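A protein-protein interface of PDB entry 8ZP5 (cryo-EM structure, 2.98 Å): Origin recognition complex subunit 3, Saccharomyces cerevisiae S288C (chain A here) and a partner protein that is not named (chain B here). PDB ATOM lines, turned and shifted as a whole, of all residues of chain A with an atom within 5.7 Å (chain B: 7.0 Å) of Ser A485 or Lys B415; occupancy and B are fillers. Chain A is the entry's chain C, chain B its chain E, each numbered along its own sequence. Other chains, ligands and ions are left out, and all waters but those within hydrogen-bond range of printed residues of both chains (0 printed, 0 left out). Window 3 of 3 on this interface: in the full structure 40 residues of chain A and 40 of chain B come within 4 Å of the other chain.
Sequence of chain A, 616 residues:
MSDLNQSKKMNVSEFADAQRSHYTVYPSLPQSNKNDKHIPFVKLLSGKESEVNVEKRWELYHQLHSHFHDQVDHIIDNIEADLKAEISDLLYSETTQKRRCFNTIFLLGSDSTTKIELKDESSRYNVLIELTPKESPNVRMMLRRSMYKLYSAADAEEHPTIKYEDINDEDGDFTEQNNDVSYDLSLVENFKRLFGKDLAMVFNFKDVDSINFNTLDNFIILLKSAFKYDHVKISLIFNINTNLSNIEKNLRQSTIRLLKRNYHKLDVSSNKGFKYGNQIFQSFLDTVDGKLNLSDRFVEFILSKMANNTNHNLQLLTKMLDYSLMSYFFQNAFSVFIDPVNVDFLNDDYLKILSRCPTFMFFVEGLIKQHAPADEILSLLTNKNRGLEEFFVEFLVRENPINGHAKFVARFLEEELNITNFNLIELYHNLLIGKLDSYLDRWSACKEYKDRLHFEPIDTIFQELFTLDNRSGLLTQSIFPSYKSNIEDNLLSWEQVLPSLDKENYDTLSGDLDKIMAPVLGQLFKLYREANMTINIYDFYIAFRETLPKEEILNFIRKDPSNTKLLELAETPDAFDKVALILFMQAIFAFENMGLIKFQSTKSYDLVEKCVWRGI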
ATOM      1  N   SER A 482       6.422  11.440  10.417  1.00  0.00           N
ATOM      2  CA  SER A 482       6.450  12.744  11.075  1.00  0.00           C
ATOM      3  C   SER A 482       6.314  13.795   9.982  1.00  0.00           C
ATOM      4  O   SER A 482       7.299  14.271   9.422  1.00  0.00           O
ATOM      5  CB  SER A 482       7.728  12.916  11.883  1.00  0.00           C
ATOM      6  OG  SER A 482       7.847  11.903  12.867  1.00  0.00           O
ATOM      7  N   TYR A 483       5.066  14.149   9.672  1.00  0.00           N
ATOM      8  CA  TYR A 483       4.778  15.090   8.594  1.00  0.00           C
ATOM      9  C   TYR A 483       5.491  16.420   8.816  1.00  0.00           C
ATOM     10  O   TYR A 483       6.346  16.832   8.019  1.00  0.00           O
ATOM     11  CB  TYR A 483       3.265  15.292   8.502  1.00  0.00           C
ATOM     12  CG  TYR A 483       2.753  15.860   7.201  1.00  0.00           C
ATOM     13  CD1 TYR A 483       2.811  17.222   6.945  1.00  0.00           C
ATOM     14  CD2 TYR A 483       2.185  15.038   6.240  1.00  0.00           C
ATOM     15  CE1 TYR A 483       2.332  17.745   5.764  1.00  0.00           C
ATOM     16  CE2 TYR A 483       1.704  15.553   5.055  1.00  0.00           C
ATOM     17  CZ  TYR A 483       1.782  16.908   4.823  1.00  0.00           C
ATOM     18  OH  TYR A 483       1.307  17.431   3.645  1.00  0.00           O
ATOM     19  N   LYS A 484       5.147  17.101   9.911  1.00  0.00           N
ATOM     20  CA  LYS A 484       5.739  18.400  10.206  1.00  0.00           C
ATOM     21  C   LYS A 484       7.250  18.293  10.346  1.00  0.00           C
ATOM     22  O   LYS A 484       7.995  19.116   9.805  1.00  0.00           O
ATOM     23  CB  LYS A 484       5.130  18.972  11.485  1.00  0.00           C
ATOM     24  CG  LYS A 484       3.829  19.719  11.287  1.00  0.00           C
ATOM     25  CD  LYS A 484       3.181  20.075  12.614  1.00  0.00           C
ATOM     26  CE  LYS A 484       4.213  20.339  13.696  1.00  0.00           C
ATOM     27  NZ  LYS A 484       4.964  21.603  13.465  1.00  0.00           N
ATOM     28  N   SER A 485       7.717  17.284  11.084  1.00  0.00           N
ATOM     29  CA  SER A 485       9.149  17.142  11.320  1.00  0.00           C
ATOM     30  C   SER A 485       9.901  16.887  10.021  1.00  0.00           C
ATOM     31  O   SER A 485      10.970  17.462   9.796  1.00  0.00           O
ATOM     32  CB  SER A 485       9.404  16.019  12.322  1.00  0.00           C
ATOM     33  OG  SER A 485       8.600  16.180  13.477  1.00  0.00           O
ATOM     34  N   ASN A 486       9.358  16.031   9.152  1.00  0.00           N
ATOM     35  CA  ASN A 486      10.025  15.761   7.881  1.00  0.00           C
ATOM     36  C   ASN A 486      10.074  17.005   7.007  1.00  0.00           C
ATOM     37  O   ASN A 486      11.110  17.302   6.398  1.00  0.00           O
ATOM     38  CB  ASN A 486       9.326  14.618   7.144  1.00  0.00           C
ATOM     39  CG  ASN A 486       9.665  13.260   7.721  1.00  0.00           C
ATOM     40  OD1 ASN A 486      10.833  12.892   7.827  1.00  0.00           O
ATOM     41  ND2 ASN A 486       8.640  12.506   8.099  1.00  0.00           N
ATOM     42  N   ILE A 487       8.970  17.754   6.937  1.00  0.00           N
ATOM     43  CA  ILE A 487       8.967  18.961   6.112  1.00  0.00           C
ATOM     44  C   ILE A 487       9.956  19.986   6.657  1.00  0.00           C
ATOM     45  O   ILE A 487      10.704  20.616   5.898  1.00  0.00           O
ATOM     46  CB  ILE A 487       7.545  19.540   6.008  1.00  0.00           C
ATOM     47  CG1 ILE A 487       6.649  18.597   5.204  1.00  0.00           C
ATOM     48  CG2 ILE A 487       7.574  20.918   5.367  1.00  0.00           C
ATOM     49  CD1 ILE A 487       5.335  19.211   4.791  1.00  0.00           C
ATOM     50  N   GLU A 488       9.990  20.159   7.981  1.00  0.00           N
ATOM     51  CA  GLU A 488      10.894  21.140   8.574  1.00  0.00           C
ATOM     52  C   GLU A 488      12.350  20.720   8.421  1.00  0.00           C
ATOM     53  O   GLU A 488      13.228  21.571   8.248  1.00  0.00           O
ATOM     54  CB  GLU A 488      10.545  21.352  10.045  1.00  0.00           C
ATOM     55  CG  GLU A 488       9.220  22.056  10.265  1.00  0.00           C
ATOM     56  CD  GLU A 488       8.495  21.552  11.492  1.00  0.00           C
ATOM     57  OE1 GLU A 488       9.166  21.257  12.502  1.00  0.00           O
ATOM     58  OE2 GLU A 488       7.253  21.431  11.443  1.00  0.00           O
ATOM     59  N   ASP A 489      12.633  19.418   8.494  1.00  0.00           N
ATOM     60  CA  ASP A 489      13.997  18.952   8.278  1.00  0.00           C
ATOM     61  C   ASP A 489      14.415  19.129   6.825  1.00  0.00           C
ATOM     62  O   ASP A 489      15.577  19.442   6.543  1.00  0.00           O
ATOM     63  CB  ASP A 489      14.129  17.491   8.704  1.00  0.00           C
ATOM     64  CG  ASP A 489      13.983  17.307  10.199  1.00  0.00           C
ATOM     65  OD1 ASP A 489      14.260  18.269  10.946  1.00  0.00           O
ATOM     66  OD2 ASP A 489      13.591  16.202  10.628  1.00  0.00           O
ATOM     67  N   ASN A 490      13.487  18.920   5.887  1.00  0.00           N
ATOM     68  CA  ASN A 490      13.787  19.198   4.487  1.00  0.00           C
ATOM     69  C   ASN A 490      14.081  20.676   4.275  1.00  0.00           C
ATOM     70  O   ASN A 490      15.005  21.035   3.538  1.00  0.00           O
ATOM     71  CB  ASN A 490      12.627  18.754   3.598  1.00  0.00           C
ATOM     72  CG  ASN A 490      12.426  17.256   3.608  1.00  0.00           C
ATOM     73  OD1 ASN A 490      11.339  16.761   3.310  1.00  0.00           O
ATOM     74  ND2 ASN A 490      13.473  16.524   3.957  1.00  0.00           N
ATOM     75  N   GLY A 615      10.507  20.709  15.774  1.00  0.00           N
ATOM     76  CA  GLY A 615      10.489  19.750  16.868  1.00  0.00           C
ATOM     77  C   GLY A 615       9.327  19.895  17.825  1.00  0.00           C
ATOM     78  O   GLY A 615       9.490  19.676  19.032  1.00  0.00           O
ATOM     79  N   ILE A 616       8.153  20.257  17.318  1.00  0.00           N
ATOM     80  CA  ILE A 616       6.967  20.371  18.158  1.00  0.00           C
ATOM     81  C   ILE A 616       5.836  19.532  17.579  1.00  0.00           C
ATOM     82  O   ILE A 616       5.115  18.841  18.300  1.00  0.00           O
ATOM     83  CB  ILE A 616       6.538  21.840  18.322  1.00  0.00           C
ATOM     84  CG1 ILE A 616       7.522  22.581  19.227  1.00  0.00           C
ATOM     85  CG2 ILE A 616       5.131  21.933  18.888  1.00  0.00           C
ATOM     86  CD1 ILE A 616       7.182  24.033  19.426  1.00  0.00           C
ATOM     87  OXT ILE A 616       5.624  19.516  16.368  1.00  0.00           O
ATOM     88  N   ILE B 327      -2.658   9.225  23.600  1.00  0.00           N
ATOM     89  CA  ILE B 327      -2.430  10.448  22.838  1.00  0.00           C
ATOM     90  C   ILE B 327      -3.654  11.349  22.903  1.00  0.00           C
ATOM     91  O   ILE B 327      -3.538  12.559  23.113  1.00  0.00           O
ATOM     92  CB  ILE B 327      -2.052  10.119  21.383  1.00  0.00           C
ATOM     93  CG1 ILE B 327      -0.624   9.583  21.306  1.00  0.00           C
ATOM     94  CG2 ILE B 327      -2.190  11.349  20.506  1.00  0.00           C
ATOM     95  CD1 ILE B 327      -0.145   9.356  19.893  1.00  0.00           C
ATOM     96  N   PHE B 390       1.138  19.964  24.588  1.00  0.00           N
ATOM     97  CA  PHE B 390       1.079  18.509  24.515  1.00  0.00           C
ATOM     98  C   PHE B 390       2.472  17.900  24.587  1.00  0.00           C
ATOM     99  O   PHE B 390       2.686  16.902  25.284  1.00  0.00           O
ATOM    100  CB  PHE B 390       0.363  18.092  23.228  1.00  0.00           C
ATOM    101  CG  PHE B 390       0.478  16.630  22.905  1.00  0.00           C
ATOM    102  CD1 PHE B 390      -0.361  15.707  23.503  1.00  0.00           C
ATOM    103  CD2 PHE B 390       1.408  16.182  21.983  1.00  0.00           C
ATOM    104  CE1 PHE B 390      -0.264  14.365  23.200  1.00  0.00           C
ATOM    105  CE2 PHE B 390       1.511  14.841  21.678  1.00  0.00           C
ATOM    106  CZ  PHE B 390       0.673  13.931  22.288  1.00  0.00           C
ATOM    107  N   GLN B 391       3.433  18.489  23.874  1.00  0.00           N
ATOM    108  CA  GLN B 391       4.812  18.020  23.959  1.00  0.00           C
ATOM    109  C   GLN B 391       5.386  18.246  25.352  1.00  0.00           C
ATOM    110  O   GLN B 391       6.143  17.411  25.862  1.00  0.00           O
ATOM    111  CB  GLN B 391       5.667  18.716  22.901  1.00  0.00           C
ATOM    112  CG  GLN B 391       7.159  18.484  23.050  1.00  0.00           C
ATOM    113  CD  GLN B 391       7.885  18.524  21.723  1.00  0.00           C
ATOM    114  OE1 GLN B 391       7.275  18.383  20.666  1.00  0.00           O
ATOM    115  NE2 GLN B 391       9.197  18.719  21.771  1.00  0.00           N
ATOM    116  N   SER B 412      14.049  12.256  22.810  1.00  0.00           N
ATOM    117  CA  SER B 412      13.451  11.986  24.113  1.00  0.00           C
ATOM    118  C   SER B 412      12.156  12.769  24.296  1.00  0.00           C
ATOM    119  O   SER B 412      11.670  12.928  25.415  1.00  0.00           O
ATOM    120  CB  SER B 412      14.435  12.325  25.235  1.00  0.00           C
ATOM    121  OG  SER B 412      15.458  11.349  25.326  1.00  0.00           O
ATOM    122  N   LEU B 413      11.603  13.257  23.189  1.00  0.00           N
ATOM    123  CA  LEU B 413      10.358  14.009  23.199  1.00  0.00           C
ATOM    124  C   LEU B 413       9.457  13.506  22.082  1.00  0.00           C
ATOM    125  O   LEU B 413       9.928  12.965  21.078  1.00  0.00           O
ATOM    126  CB  LEU B 413      10.604  15.514  23.036  1.00  0.00           C
ATOM    127  CG  LEU B 413      10.831  16.299  24.329  1.00  0.00           C
ATOM    128  CD1 LEU B 413      11.442  17.656  24.028  1.00  0.00           C
ATOM    129  CD2 LEU B 413       9.529  16.449  25.098  1.00  0.00           C
ATOM    130  N   MET B 414       8.153  13.690  22.265  1.00  0.00           N
ATOM    131  CA  MET B 414       7.165  13.200  21.315  1.00  0.00           C
ATOM    132  C   MET B 414       6.891  14.264  20.262  1.00  0.00           C
ATOM    133  O   MET B 414       6.411  15.356  20.584  1.00  0.00           O
ATOM    134  CB  MET B 414       5.872  12.809  22.029  1.00  0.00           C
ATOM    135  CG  MET B 414       4.773  12.373  21.082  1.00  0.00           C
ATOM    136  SD  MET B 414       4.758  10.591  20.825  1.00  0.00           S
ATOM    137  CE  MET B 414       3.278  10.414  19.836  1.00  0.00           C
ATOM    138  N   LYS B 415       7.194  13.943  19.008  1.00  0.00           N
ATOM    139  CA  LYS B 415       6.909  14.831  17.894  1.00  0.00           C
ATOM    140  C   LYS B 415       5.459  14.668  17.443  1.00  0.00           C
ATOM    141  O   LYS B 415       4.748  13.749  17.856  1.00  0.00           O
ATOM    142  CB  LYS B 415       7.865  14.556  16.734  1.00  0.00           C
ATOM    143  CG  LYS B 415       9.310  14.921  17.025  1.00  0.00           C
ATOM    144  CD  LYS B 415      10.203  14.620  15.835  1.00  0.00           C
ATOM    145  CE  LYS B 415      11.630  15.078  16.087  1.00  0.00           C
ATOM    146  NZ  LYS B 415      12.279  14.293  17.171  1.00  0.00           N
ATOM    147  N   ALA B 416       5.017  15.588  16.591  1.00  0.00           N
ATOM    148  CA  ALA B 416       3.660  15.559  16.048  1.00  0.00           C
ATOM    149  C   ALA B 416       3.648  14.656  14.821  1.00  0.00           C
ATOM    150  O   ALA B 416       3.958  15.093  13.710  1.00  0.00           O
ATOM    151  CB  ALA B 416       3.184  16.968  15.711  1.00  0.00           C
ATOM    152  N   ASN B 417       3.287  13.391  15.020  1.00  0.00           N
ATOM    153  CA  ASN B 417       3.191  12.437  13.923  1.00  0.00           C
ATOM    154  C   ASN B 417       1.874  12.642  13.181  1.00  0.00           C
ATOM    155  O   ASN B 417       1.125  13.590  13.434  1.00  0.00           O
ATOM    156  CB  ASN B 417       3.312  11.007  14.442  1.00  0.00           C
ATOM    157  CG  ASN B 417       4.521  10.804  15.325  1.00  0.00           C
ATOM    158  OD1 ASN B 417       4.638  11.413  16.386  1.00  0.00           O
ATOM    159  ND2 ASN B 417       5.429   9.936  14.894  1.00  0.00           N
ATOM    160  N   ILE B 418       1.581  11.744  12.239  1.00  0.00           N
ATOM    161  CA  ILE B 418       0.243  11.686  11.660  1.00  0.00           C
ATOM    162  C   ILE B 418      -0.759  11.255  12.716  1.00  0.00           C
ATOM    163  O   ILE B 418      -1.913  11.700  12.712  1.00  0.00           O
ATOM    164  CB  ILE B 418       0.223  10.730  10.453  1.00  0.00           C
ATOM    165  CG1 ILE B 418       1.274  11.146   9.431  1.00  0.00           C
ATOM    166  CG2 ILE B 418      -1.150  10.709   9.808  1.00  0.00           C
ATOM    167  CD1 ILE B 418       1.061  12.504   8.861  1.00  0.00           C
ATOM    168  N   VAL B 420      -0.889  11.859  15.972  1.00  0.00           N
ATOM    169  CA  VAL B 420      -1.310  12.931  16.871  1.00  0.00           C
ATOM    170  C   VAL B 420      -2.376  13.796  16.209  1.00  0.00           C
ATOM    171  O   VAL B 420      -3.397  14.137  16.820  1.00  0.00           O
ATOM    172  CB  VAL B 420      -0.095  13.770  17.307  1.00  0.00           C
ATOM    173  CG1 VAL B 420      -0.543  15.101  17.883  1.00  0.00           C
ATOM    174  CG2 VAL B 420       0.743  13.003  18.315  1.00  0.00           C
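OE1 of Gln B391 lies close to O of Ile A616.
The side-chain amide nitrogen of Gln B391 sits at hydrogen-bond distance from the backbone carbonyl oxygen of Gly A615 (2.9 Å).
The side-chain amide nitrogen (ND2) of Asn A486 sits at hydrogen-bond distance from the backbone carbonyl oxygen (O) of Ser A482, 2.6 Å away.
The backbone carbonyl oxygen (O) of Lys B415 sits close to the side-chain amide oxygen (OD1) of Asn B417 (2.8 Å).
OE1 of Gln B391 sits close to O of Met B414 (3.1 Å).
The side-chain amino group (NZ) of Lys A484 is in salt-bridge range of the chain-end carboxylate (OXT) of Ile A616.
Among the printed residues, merely in contact across the chains: Ser A485 with Lys B415, Tyr A483 with Ile B418, Ile A616 with Ala B416 and Ser A482 with Asn B417.
Ser A485 touches one residue of chain B.
Of chain A, only Ser A485 comes within 4 Å of Lys B415.
Of the printed residues of chain B, Tyr A483 touches Ile B418.
Of the printed residues of chain A, Asn B417 touches Ser A482 (3.7 Å).
Of the printed residues of chain A, Ile B418 touches Tyr A483 (3.6 Å).
The nearest printed residue of chain A that does not touch Gln B391 is Ser A485 (7.6 Å).
Of the 11 printed residues of chain A, 5 touch a printed residue of chain B.
Printed residues of chain A that touch a printed residue of chain B: Ser A482, Tyr A483, Ser A485, Gly A615 and Ile A616.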
